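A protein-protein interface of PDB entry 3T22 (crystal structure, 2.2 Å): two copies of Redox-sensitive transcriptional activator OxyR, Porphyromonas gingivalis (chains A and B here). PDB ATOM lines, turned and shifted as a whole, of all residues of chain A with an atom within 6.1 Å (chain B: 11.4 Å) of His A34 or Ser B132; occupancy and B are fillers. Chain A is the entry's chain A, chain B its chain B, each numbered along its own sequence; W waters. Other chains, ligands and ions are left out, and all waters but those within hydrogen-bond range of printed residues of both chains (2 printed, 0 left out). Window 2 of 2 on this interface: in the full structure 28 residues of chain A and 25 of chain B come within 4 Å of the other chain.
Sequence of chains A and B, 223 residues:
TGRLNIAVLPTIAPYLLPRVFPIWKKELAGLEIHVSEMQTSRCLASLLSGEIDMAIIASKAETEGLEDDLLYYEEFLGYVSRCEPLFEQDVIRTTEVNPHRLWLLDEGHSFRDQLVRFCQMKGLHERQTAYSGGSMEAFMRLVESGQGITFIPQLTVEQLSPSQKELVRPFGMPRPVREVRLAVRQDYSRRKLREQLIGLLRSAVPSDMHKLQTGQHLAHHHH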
ATOM      1  N   ARG A   3      35.940 -10.723 -13.722  1.00  0.00           N
ATOM      2  CA  ARG A   3      35.063 -10.200 -14.765  1.00  0.00           C
ATOM      3  C   ARG A   3      35.471  -8.765 -15.065  1.00  0.00           C
ATOM      4  O   ARG A   3      36.242  -8.172 -14.311  1.00  0.00           O
ATOM      5  CB  ARG A   3      33.602 -10.237 -14.309  1.00  0.00           C
ATOM      6  CG  ARG A   3      33.292  -9.428 -13.035  1.00  0.00           C
ATOM      7  CD  ARG A   3      31.856  -9.706 -12.558  1.00  0.00           C
ATOM      8  NE  ARG A   3      31.514  -9.040 -11.303  1.00  0.00           N
ATOM      9  CZ  ARG A   3      30.718  -7.978 -11.216  1.00  0.00           C
ATOM     10  NH1 ARG A   3      30.183  -7.465 -12.316  1.00  0.00           N
ATOM     11  NH2 ARG A   3      30.451  -7.429 -10.035  1.00  0.00           N
ATOM     12  N   LEU A   4      34.965  -8.205 -16.161  1.00  0.00           N
ATOM     13  CA  LEU A   4      35.241  -6.809 -16.464  1.00  0.00           C
ATOM     14  C   LEU A   4      34.092  -5.892 -16.040  1.00  0.00           C
ATOM     15  O   LEU A   4      32.976  -6.025 -16.513  1.00  0.00           O
ATOM     16  CB  LEU A   4      35.565  -6.618 -17.948  1.00  0.00           C
ATOM     17  CG  LEU A   4      36.204  -5.278 -18.344  1.00  0.00           C
ATOM     18  CD1 LEU A   4      37.497  -5.031 -17.556  1.00  0.00           C
ATOM     19  CD2 LEU A   4      36.470  -5.202 -19.836  1.00  0.00           C
ATOM     20  N   ASN A   5      34.374  -4.958 -15.144  1.00  0.00           N
ATOM     21  CA  ASN A   5      33.402  -3.935 -14.800  1.00  0.00           C
ATOM     22  C   ASN A   5      33.642  -2.659 -15.582  1.00  0.00           C
ATOM     23  O   ASN A   5      34.576  -1.908 -15.280  1.00  0.00           O
ATOM     24  CB  ASN A   5      33.440  -3.643 -13.303  1.00  0.00           C
ATOM     25  CG  ASN A   5      32.878  -4.788 -12.476  1.00  0.00           C
ATOM     26  OD1 ASN A   5      31.986  -5.511 -12.936  1.00  0.00           O
ATOM     27  ND2 ASN A   5      33.405  -4.970 -11.260  1.00  0.00           N
ATOM     28  N   ILE A   6      32.804  -2.397 -16.584  1.00  0.00           N
ATOM     29  CA  ILE A   6      32.983  -1.196 -17.392  1.00  0.00           C
ATOM     30  C   ILE A   6      31.792  -0.242 -17.350  1.00  0.00           C
ATOM     31  O   ILE A   6      30.654  -0.659 -17.500  1.00  0.00           O
ATOM     32  CB  ILE A   6      33.408  -1.544 -18.847  1.00  0.00           C
ATOM     33  CG1 ILE A   6      33.463  -0.296 -19.731  1.00  0.00           C
ATOM     34  CG2 ILE A   6      32.503  -2.566 -19.450  1.00  0.00           C
ATOM     35  CD1 ILE A   6      34.046  -0.611 -21.083  1.00  0.00           C
ATOM     36  N   ALA A   7      32.065   1.040 -17.137  1.00  0.00           N
ATOM     37  CA  ALA A   7      31.022   2.061 -17.137  1.00  0.00           C
ATOM     38  C   ALA A   7      30.953   2.851 -18.448  1.00  0.00           C
ATOM     39  O   ALA A   7      31.936   2.941 -19.197  1.00  0.00           O
ATOM     40  CB  ALA A   7      31.198   3.011 -15.955  1.00  0.00           C
ATOM     41  N   GLU A  32      33.208 -12.420 -18.959  1.00  0.00           N
ATOM     42  CA  GLU A  32      31.932 -11.958 -18.422  1.00  0.00           C
ATOM     43  C   GLU A  32      31.975 -10.470 -18.109  1.00  0.00           C
ATOM     44  O   GLU A  32      32.637 -10.038 -17.166  1.00  0.00           O
ATOM     45  CB  GLU A  32      31.579 -12.740 -17.165  1.00  0.00           C
ATOM     46  CG  GLU A  32      32.755 -12.926 -16.218  1.00  0.00           C
ATOM     47  CD  GLU A  32      32.388 -13.720 -14.980  1.00  0.00           C
ATOM     48  OE1 GLU A  32      31.175 -14.008 -14.802  1.00  0.00           O
ATOM     49  OE2 GLU A  32      33.313 -14.050 -14.194  1.00  0.00           O
ATOM     50  N   ILE A  33      31.250  -9.694 -18.902  1.00  0.00           N
ATOM     51  CA  ILE A  33      31.295  -8.241 -18.819  1.00  0.00           C
ATOM     52  C   ILE A  33      30.073  -7.691 -18.095  1.00  0.00           C
ATOM     53  O   ILE A  33      28.956  -8.165 -18.297  1.00  0.00           O
ATOM     54  CB  ILE A  33      31.372  -7.615 -20.231  1.00  0.00           C
ATOM     55  CG1 ILE A  33      32.645  -8.066 -20.952  1.00  0.00           C
ATOM     56  CG2 ILE A  33      31.313  -6.093 -20.164  1.00  0.00           C
ATOM     57  CD1 ILE A  33      32.938  -7.277 -22.206  1.00  0.00           C
ATOM     58  N   HIS A  34      30.290  -6.697 -17.243  1.00  0.00           N
ATOM     59  CA  HIS A  34      29.191  -6.008 -16.601  1.00  0.00           C
ATOM     60  C   HIS A  34      29.233  -4.549 -16.950  1.00  0.00           C
ATOM     61  O   HIS A  34      30.202  -3.859 -16.652  1.00  0.00           O
ATOM     62  CB  HIS A  34      29.241  -6.158 -15.087  1.00  0.00           C
ATOM     63  CG  HIS A  34      28.262  -5.275 -14.372  1.00  0.00           C
ATOM     64  ND1 HIS A  34      28.649  -4.185 -13.618  1.00  0.00           N
ATOM     65  CD2 HIS A  34      26.907  -5.302 -14.321  1.00  0.00           C
ATOM     66  CE1 HIS A  34      27.577  -3.590 -13.124  1.00  0.00           C
ATOM     67  NE2 HIS A  34      26.507  -4.248 -13.537  1.00  0.00           N
ATOM     68  N   VAL A  35      28.173  -4.069 -17.574  1.00  0.00           N
ATOM     69  CA  VAL A  35      28.103  -2.672 -17.980  1.00  0.00           C
ATOM     70  C   VAL A  35      27.250  -1.881 -16.991  1.00  0.00           C
ATOM     71  O   VAL A  35      26.256  -2.385 -16.507  1.00  0.00           O
ATOM     72  CB  VAL A  35      27.512  -2.549 -19.394  1.00  0.00           C
ATOM     73  CG1 VAL A  35      27.372  -1.101 -19.783  1.00  0.00           C
ATOM     74  CG2 VAL A  35      28.384  -3.277 -20.370  1.00  0.00           C
ATOM     75  N   SER A  36      27.632  -0.647 -16.702  1.00  0.00           N
ATOM     76  CA  SER A  36      26.839   0.224 -15.848  1.00  0.00           C
ATOM     77  C   SER A  36      26.763   1.589 -16.491  1.00  0.00           C
ATOM     78  O   SER A  36      27.810   2.127 -16.901  1.00  0.00           O
ATOM     79  CB  SER A  36      27.475   0.382 -14.464  1.00  0.00           C
ATOM     80  OG  SER A  36      28.314  -0.696 -14.127  1.00  0.00           O
ATOM     81  N   GLU A  37      25.560   2.162 -16.574  1.00  0.00           N
ATOM     82  CA  GLU A  37      25.444   3.551 -17.026  1.00  0.00           C
ATOM     83  C   GLU A  37      25.747   4.561 -15.885  1.00  0.00           C
ATOM     84  O   GLU A  37      25.155   4.483 -14.834  1.00  0.00           O
ATOM     85  CB  GLU A  37      24.086   3.827 -17.688  1.00  0.00           C
ATOM     86  CG  GLU A  37      24.000   3.419 -19.160  1.00  0.00           C
ATOM     87  CD  GLU A  37      22.610   3.658 -19.807  1.00  0.00           C
ATOM     88  OE1 GLU A  37      22.187   4.820 -19.926  1.00  0.00           O
ATOM     89  OE2 GLU A  37      21.950   2.680 -20.222  1.00  0.00           O
ATOM     90  N   GLN B  39      12.290   9.732 -10.060  1.00  0.00           N
ATOM     91  CA  GLN B  39      11.704   8.450  -9.740  1.00  0.00           C
ATOM     92  C   GLN B  39      10.643   8.624  -8.666  1.00  0.00           C
ATOM     93  O   GLN B  39      10.419   9.729  -8.182  1.00  0.00           O
ATOM     94  CB  GLN B  39      12.782   7.447  -9.342  1.00  0.00           C
ATOM     95  CG  GLN B  39      13.502   6.876 -10.549  1.00  0.00           C
ATOM     96  CD  GLN B  39      14.668   5.998 -10.181  1.00  0.00           C
ATOM     97  OE1 GLN B  39      14.550   5.110  -9.342  1.00  0.00           O
ATOM     98  NE2 GLN B  39      15.805   6.235 -10.814  1.00  0.00           N
ATOM     99  N   HIS B 100      18.965 -14.479 -18.936  1.00  0.00           N
ATOM    100  CA  HIS B 100      20.331 -14.044 -19.186  1.00  0.00           C
ATOM    101  C   HIS B 100      20.361 -13.156 -20.426  1.00  0.00           C
ATOM    102  O   HIS B 100      21.350 -12.468 -20.696  1.00  0.00           O
ATOM    103  CB  HIS B 100      21.260 -15.254 -19.326  1.00  0.00           C
ATOM    104  CG  HIS B 100      21.248 -16.157 -18.126  1.00  0.00           C
ATOM    105  ND1 HIS B 100      20.127 -16.862 -17.736  1.00  0.00           N
ATOM    106  CD2 HIS B 100      22.212 -16.451 -17.221  1.00  0.00           C
ATOM    107  CE1 HIS B 100      20.406 -17.563 -16.651  1.00  0.00           C
ATOM    108  NE2 HIS B 100      21.664 -17.333 -16.317  1.00  0.00           N
ATOM    109  N   LEU B 102      17.768 -10.827 -20.885  1.00  0.00           N
ATOM    110  CA  LEU B 102      16.667  -9.926 -20.544  1.00  0.00           C
ATOM    111  C   LEU B 102      17.136  -8.587 -19.941  1.00  0.00           C
ATOM    112  O   LEU B 102      17.785  -8.577 -18.886  1.00  0.00           O
ATOM    113  CB  LEU B 102      15.726 -10.628 -19.568  1.00  0.00           C
ATOM    114  CG  LEU B 102      14.514  -9.862 -19.058  1.00  0.00           C
ATOM    115  CD1 LEU B 102      13.497  -9.626 -20.199  1.00  0.00           C
ATOM    116  CD2 LEU B 102      13.855 -10.595 -17.851  1.00  0.00           C
ATOM    117  N   TRP B 103      16.783  -7.469 -20.591  1.00  0.00           N
ATOM    118  CA  TRP B 103      17.116  -6.126 -20.089  1.00  0.00           C
ATOM    119  C   TRP B 103      16.072  -5.579 -19.115  1.00  0.00           C
ATOM    120  O   TRP B 103      14.907  -5.363 -19.474  1.00  0.00           O
ATOM    121  CB  TRP B 103      17.289  -5.126 -21.242  1.00  0.00           C
ATOM    122  CG  TRP B 103      18.083  -5.654 -22.382  1.00  0.00           C
ATOM    123  CD1 TRP B 103      17.643  -5.881 -23.657  1.00  0.00           C
ATOM    124  CD2 TRP B 103      19.455  -6.042 -22.358  1.00  0.00           C
ATOM    125  NE1 TRP B 103      18.661  -6.393 -24.427  1.00  0.00           N
ATOM    126  CE2 TRP B 103      19.785  -6.502 -23.650  1.00  0.00           C
ATOM    127  CE3 TRP B 103      20.441  -6.052 -21.371  1.00  0.00           C
ATOM    128  CZ2 TRP B 103      21.059  -6.951 -23.978  1.00  0.00           C
ATOM    129  CZ3 TRP B 103      21.702  -6.514 -21.693  1.00  0.00           C
ATOM    130  CH2 TRP B 103      22.003  -6.947 -22.985  1.00  0.00           C
ATOM    131  N   LEU B 104      16.499  -5.337 -17.883  1.00  0.00           N
ATOM    132  CA  LEU B 104      15.603  -4.804 -16.866  1.00  0.00           C
ATOM    133  C   LEU B 104      16.162  -3.493 -16.329  1.00  0.00           C
ATOM    134  O   LEU B 104      17.381  -3.331 -16.223  1.00  0.00           O
ATOM    135  CB  LEU B 104      15.414  -5.820 -15.724  1.00  0.00           C
ATOM    136  CG  LEU B 104      14.276  -6.848 -15.830  1.00  0.00           C
ATOM    137  CD1 LEU B 104      14.504  -8.053 -14.919  1.00  0.00           C
ATOM    138  CD2 LEU B 104      12.924  -6.220 -15.519  1.00  0.00           C
ATOM    139  N   LEU B 105      15.275  -2.558 -16.001  1.00  0.00           N
ATOM    140  CA  LEU B 105      15.677  -1.321 -15.340  1.00  0.00           C
ATOM    141  C   LEU B 105      16.085  -1.607 -13.886  1.00  0.00           C
ATOM    142  O   LEU B 105      15.792  -2.685 -13.352  1.00  0.00           O
ATOM    143  CB  LEU B 105      14.534  -0.318 -15.355  1.00  0.00           C
ATOM    144  CG  LEU B 105      14.019   0.212 -16.692  1.00  0.00           C
ATOM    145  CD1 LEU B 105      12.723   0.975 -16.474  1.00  0.00           C
ATOM    146  CD2 LEU B 105      15.057   1.093 -17.416  1.00  0.00           C
ATOM    147  N   ASP B 106      16.741  -0.638 -13.246  1.00  0.00           N
ATOM    148  CA  ASP B 106      17.180  -0.803 -11.859  1.00  0.00           C
ATOM    149  C   ASP B 106      16.003  -0.848 -10.877  1.00  0.00           C
ATOM    150  O   ASP B 106      15.013  -0.131 -11.052  1.00  0.00           O
ATOM    151  CB  ASP B 106      18.126   0.324 -11.449  1.00  0.00           C
ATOM    152  CG  ASP B 106      19.529   0.150 -12.008  1.00  0.00           C
ATOM    153  OD1 ASP B 106      19.863  -0.939 -12.514  1.00  0.00           O
ATOM    154  OD2 ASP B 106      20.314   1.114 -11.909  1.00  0.00           O
ATOM    155  N   GLU B 107      16.127  -1.688  -9.848  1.00  0.00           N
ATOM    156  CA  GLU B 107      15.227  -1.658  -8.689  1.00  0.00           C
ATOM    157  C   GLU B 107      15.021  -0.249  -8.173  1.00  0.00           C
ATOM    158  O   GLU B 107      15.984   0.471  -7.946  1.00  0.00           O
ATOM    159  CB  GLU B 107      15.829  -2.451  -7.550  1.00  0.00           C
ATOM    160  CG  GLU B 107      15.758  -3.930  -7.718  1.00  0.00           C
ATOM    161  CD  GLU B 107      16.092  -4.631  -6.417  1.00  0.00           C
ATOM    162  OE1 GLU B 107      17.300  -4.927  -6.201  1.00  0.00           O
ATOM    163  OE2 GLU B 107      15.150  -4.858  -5.609  1.00  0.00           O
ATOM    164  N   GLY B 108      13.778   0.142  -7.945  1.00  0.00           N
ATOM    165  CA  GLY B 108      13.523   1.517  -7.560  1.00  0.00           C
ATOM    166  C   GLY B 108      12.665   2.189  -8.612  1.00  0.00           C
ATOM    167  O   GLY B 108      11.863   3.076  -8.296  1.00  0.00           O
ATOM    168  N   HIS B 109      12.843   1.774  -9.868  1.00  0.00           N
ATOM    169  CA  HIS B 109      11.883   2.096 -10.923  1.00  0.00           C
ATOM    170  C   HIS B 109      10.660   1.201 -10.715  1.00  0.00           C
ATOM    171  O   HIS B 109      10.770  -0.032 -10.719  1.00  0.00           O
ATOM    172  CB  HIS B 109      12.475   1.827 -12.313  1.00  0.00           C
ATOM    173  CG  HIS B 109      13.566   2.772 -12.701  1.00  0.00           C
ATOM    174  ND1 HIS B 109      13.320   3.953 -13.370  1.00  0.00           N
ATOM    175  CD2 HIS B 109      14.907   2.716 -12.509  1.00  0.00           C
ATOM    176  CE1 HIS B 109      14.465   4.587 -13.567  1.00  0.00           C
ATOM    177  NE2 HIS B 109      15.442   3.856 -13.057  1.00  0.00           N
ATOM    178  N   ARG B 112       9.943  -1.664 -13.222  1.00  0.00           N
ATOM    179  CA  ARG B 112      10.610  -2.929 -12.968  1.00  0.00           C
ATOM    180  C   ARG B 112      10.035  -3.654 -11.736  1.00  0.00           C
ATOM    181  O   ARG B 112       9.720  -4.839 -11.822  1.00  0.00           O
ATOM    182  CB  ARG B 112      12.128  -2.756 -12.847  1.00  0.00           C
ATOM    183  CG  ARG B 112      12.869  -4.024 -12.438  1.00  0.00           C
ATOM    184  CD  ARG B 112      13.370  -3.940 -11.002  1.00  0.00           C
ATOM    185  NE  ARG B 112      14.057  -5.166 -10.583  1.00  0.00           N
ATOM    186  CZ  ARG B 112      15.348  -5.433 -10.818  1.00  0.00           C
ATOM    187  NH1 ARG B 112      16.119  -4.566 -11.479  1.00  0.00           N
ATOM    188  NH2 ARG B 112      15.878  -6.573 -10.393  1.00  0.00           N
ATOM    189  N   ALA B 130      24.428  -7.927 -15.260  1.00  0.00           N
ATOM    190  CA  ALA B 130      24.810  -7.807 -16.658  1.00  0.00           C
ATOM    191  C   ALA B 130      24.828  -6.358 -17.127  1.00  0.00           C
ATOM    192  O   ALA B 130      25.773  -5.926 -17.776  1.00  0.00           O
ATOM    193  CB  ALA B 130      23.886  -8.631 -17.529  1.00  0.00           C
ATOM    194  N   TYR B 131      23.782  -5.610 -16.801  1.00  0.00           N
ATOM    195  CA  TYR B 131      23.658  -4.241 -17.264  1.00  0.00           C
ATOM    196  C   TYR B 131      22.842  -3.441 -16.257  1.00  0.00           C
ATOM    197  O   TYR B 131      21.635  -3.623 -16.140  1.00  0.00           O
ATOM    198  CB  TYR B 131      23.000  -4.213 -18.643  1.00  0.00           C
ATOM    199  CG  TYR B 131      22.997  -2.862 -19.320  1.00  0.00           C
ATOM    200  CD1 TYR B 131      22.742  -1.707 -18.603  1.00  0.00           C
ATOM    201  CD2 TYR B 131      23.236  -2.745 -20.680  1.00  0.00           C
ATOM    202  CE1 TYR B 131      22.734  -0.479 -19.214  1.00  0.00           C
ATOM    203  CE2 TYR B 131      23.227  -1.517 -21.301  1.00  0.00           C
ATOM    204  CZ  TYR B 131      22.975  -0.387 -20.561  1.00  0.00           C
ATOM    205  OH  TYR B 131      22.961   0.846 -21.164  1.00  0.00           O
ATOM    206  N   SER B 132      23.513  -2.561 -15.524  1.00  0.00           N
ATOM    207  CA  SER B 132      22.852  -1.751 -14.517  1.00  0.00           C
ATOM    208  C   SER B 132      22.813  -0.292 -14.923  1.00  0.00           C
ATOM    209  O   SER B 132      23.674   0.179 -15.656  1.00  0.00           O
ATOM    210  CB  SER B 132      23.560  -1.879 -13.170  1.00  0.00           C
ATOM    211  OG  SER B 132      24.315  -3.069 -13.090  1.00  0.00           O
ATOM    212  N   GLY B 133      21.807   0.418 -14.428  1.00  0.00           N
ATOM    213  CA  GLY B 133      21.704   1.846 -14.636  1.00  0.00           C
ATOM    214  C   GLY B 133      21.096   2.140 -15.988  1.00  0.00           C
ATOM    215  O   GLY B 133      21.039   3.298 -16.391  1.00  0.00           O
ATOM    216  N   GLY B 134      20.624   1.098 -16.677  1.00  0.00           N
ATOM    217  CA  GLY B 134      20.128   1.227 -18.040  1.00  0.00           C
ATOM    218  C   GLY B 134      18.944   2.165 -18.237  1.00  0.00           C
ATOM    219  O   GLY B 134      18.151   2.370 -17.318  1.00  0.00           O
ATOM    220  N   SER B 135      18.846   2.768 -19.422  1.00  0.00           N
ATOM    221  CA  SER B 135      17.618   3.469 -19.824  1.00  0.00           C
ATOM    222  C   SER B 135      16.792   2.633 -20.812  1.00  0.00           C
ATOM    223  O   SER B 135      17.324   1.769 -21.503  1.00  0.00           O
ATOM    224  CB  SER B 135      17.930   4.816 -20.461  1.00  0.00           C
ATOM    225  OG  SER B 135      18.610   4.634 -21.679  1.00  0.00           O
ATOM    226  N   MET B 136      15.492   2.902 -20.878  1.00  0.00           N
ATOM    227  CA  MET B 136      14.613   2.212 -21.812  1.00  0.00           C
ATOM    228  C   MET B 136      15.081   2.456 -23.239  1.00  0.00           C
ATOM    229  O   MET B 136      14.977   1.581 -24.095  1.00  0.00           O
ATOM    230  CB  MET B 136      13.174   2.705 -21.673  1.00  0.00           C
ATOM    231  CG  MET B 136      12.142   1.715 -22.215  1.00  0.00           C
ATOM    232  SD  MET B 136      11.301   0.923 -20.823  1.00  0.00           S
ATOM    233  CE  MET B 136      10.716   2.374 -19.959  1.00  0.00           C
ATOM    234  N   ALA B 138      18.190   2.759 -24.266  1.00  0.00           N
ATOM    235  CA  ALA B 138      19.243   1.769 -24.486  1.00  0.00           C
ATOM    236  C   ALA B 138      18.718   0.344 -24.760  1.00  0.00           C
ATOM    237  O   ALA B 138      19.167  -0.324 -25.695  1.00  0.00           O
ATOM    238  CB  ALA B 138      20.238   1.763 -23.319  1.00  0.00           C
ATOM    239  N   PHE B 139      17.791  -0.130 -23.933  1.00  0.00           N
ATOM    240  CA  PHE B 139      17.289  -1.496 -24.075  1.00  0.00           C
ATOM    241  C   PHE B 139      16.587  -1.686 -25.403  1.00  0.00           C
ATOM    242  O   PHE B 139      16.761  -2.705 -26.070  1.00  0.00           O
ATOM    243  CB  PHE B 139      16.345  -1.836 -22.934  1.00  0.00           C
ATOM    244  CG  PHE B 139      17.002  -1.804 -21.597  1.00  0.00           C
ATOM    245  CD1 PHE B 139      18.367  -2.005 -21.488  1.00  0.00           C
ATOM    246  CD2 PHE B 139      16.266  -1.548 -20.450  1.00  0.00           C
ATOM    247  CE1 PHE B 139      18.980  -1.981 -20.245  1.00  0.00           C
ATOM    248  CE2 PHE B 139      16.867  -1.528 -19.223  1.00  0.00           C
ATOM    249  CZ  PHE B 139      18.215  -1.746 -19.112  1.00  0.00           C
ATOM    250  N   LEU B 142      19.097  -1.954 -28.262  1.00  0.00           N
ATOM    251  CA  LEU B 142      19.675  -3.290 -28.204  1.00  0.00           C
ATOM    252  C   LEU B 142      18.784  -4.353 -28.854  1.00  0.00           C
ATOM    253  O   LEU B 142      19.257  -5.140 -29.662  1.00  0.00           O
ATOM    254  CB  LEU B 142      19.983  -3.677 -26.756  1.00  0.00           C
ATOM    255  CG  LEU B 142      21.274  -3.109 -26.167  1.00  0.00           C
ATOM    256  CD1 LEU B 142      21.333  -3.319 -24.672  1.00  0.00           C
ATOM    257  CD2 LEU B 142      22.475  -3.734 -26.838  1.00  0.00           C
HETATM  258  O   HOH W   1      20.834   6.367 -17.892  1.00  0.00           O
HETATM  259  O   HOH W   2      21.030   6.308 -21.943  1.00  0.00           O
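Ala B130 touches Ile A33.
His A34 touches Ala B130 (CA to O, 3.6 Å).
Tyr B131 touches Val A35.
Ser B132 touches Ser A36 (O to CA, 3.2 Å).
O of Gly B133 touches CB of Glu A37, 3.4 Å away.
Glu A37 touches Gly B134.
Glu A37 touches Ala B138 (OE2 to CB, 3.7 Å).
The side-chain carboxylate (OE2) of Glu A37 lies close to the side-chain hydroxyl (OH) of Tyr B131 (2.3 Å).
The backbone NH of Glu A37 is in hydrogen-bond range of the backbone carbonyl oxygen of Ser B132, at 2.9 Å.
NE2 of His A34 is in hydrogen-bond range of OG of Ser B132 (2.5 Å).
OE2 of Glu A37 lies within hydrogen-bond range of N of Ser B135, at 3.2 Å.
The backbone NH (N) of Val A35 lies within hydrogen-bond range of the backbone carbonyl oxygen (O) of Ala B130 (3.0 Å).
The backbone carbonyl oxygen (O) of Val A35 is in hydrogen-bond range of the backbone NH (N) of Ser B132 (2.9 Å).
No position is printed for both chains.
Of the 13 pairs that touch across the chains among the printed residues, none has its exchanged pair printed and touching as well.
Printed residues of chain B that touch a printed residue of chain A: Ala B130, Tyr B131, Ser B132, Gly B133, Gly B134, Ser B135 and Ala B138.
Hydrophobic or aromatic side chains of chain B that line the printed part of chain A: Tyr B131 and Ala B138.
Along chain B the printed residues that touch a printed residue of chain A span positions 130 to 138.
Among the printed residues, no Asp or Glu carboxylate lies within 4 Å of a Lys or Arg side-chain nitrogen of the other chain.
N of Gly B133 lies within hydrogen-bond range of OD2 of Asp B106, at 3.0 Å.
N of Ile A6 sits at hydrogen-bond distance from O of His A34 (3.0 Å).
The backbone NH (N) of Ser A36 is in hydrogen-bond range of the backbone carbonyl oxygen (O) of Ile A6, at 3.1 Å.
The backbone NH of His A34 is in hydrogen-bond range of the backbone carbonyl oxygen of Leu A4, 2.9 Å away.
OG of Ser B135 lies within hydrogen-bond range of N of Ala B138, at 3.2 Å.
Water W2 bridges the side-chain carboxylate (OE1) of Glu A37 and the side-chain hydroxyl (OG) of Ser B135.
Water W1 lies within hydrogen-bond range of OE1 of Glu A37 (2.9 Å) and O of Gly B133 (3.4 Å).
Printed residues of chain B within 4 Å of His A34: Ala B130 (3.6 Å) and Ser B132 (2.5 Å).
Ser B132 touches just these residues of chain A: His A34, Val A35, Ser A36 and Glu A37.
Of chain B, only Ala B130 comes within 4 Å of Ile A33.
Of chain B, only Ala B130 (3.0 Å), Tyr B131 (3.3 Å) and Ser B132 (2.9 Å) come within 4 Å of Val A35.
Of the printed residues of chain B, Ser A36 touches Ser B132.
Printed residues of chain A within 4 Å of Ser B135: Glu A37 (3.2 Å).
Printed residues of chain A within 4 Å of Ala B138: Glu A37 (3.7 Å).
Of the printed residues of chain A, Tyr B131 touches Val A35 (3.3 Å) and Glu A37 (2.3 Å).
Of the printed residues of chain A, Ala B130 touches Ile A33, His A34 and Val A35.
Leu B142 touches none of the printed residues of chain A.
Arg A3 touches none of the printed residues of chain B.
The nearest printed residue of chain B that does not touch His A34 is Tyr B131 (4.001 Å).
The nearest printed residue of chain A that does not touch Ser B132 is Ile A6 (7.3 Å).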
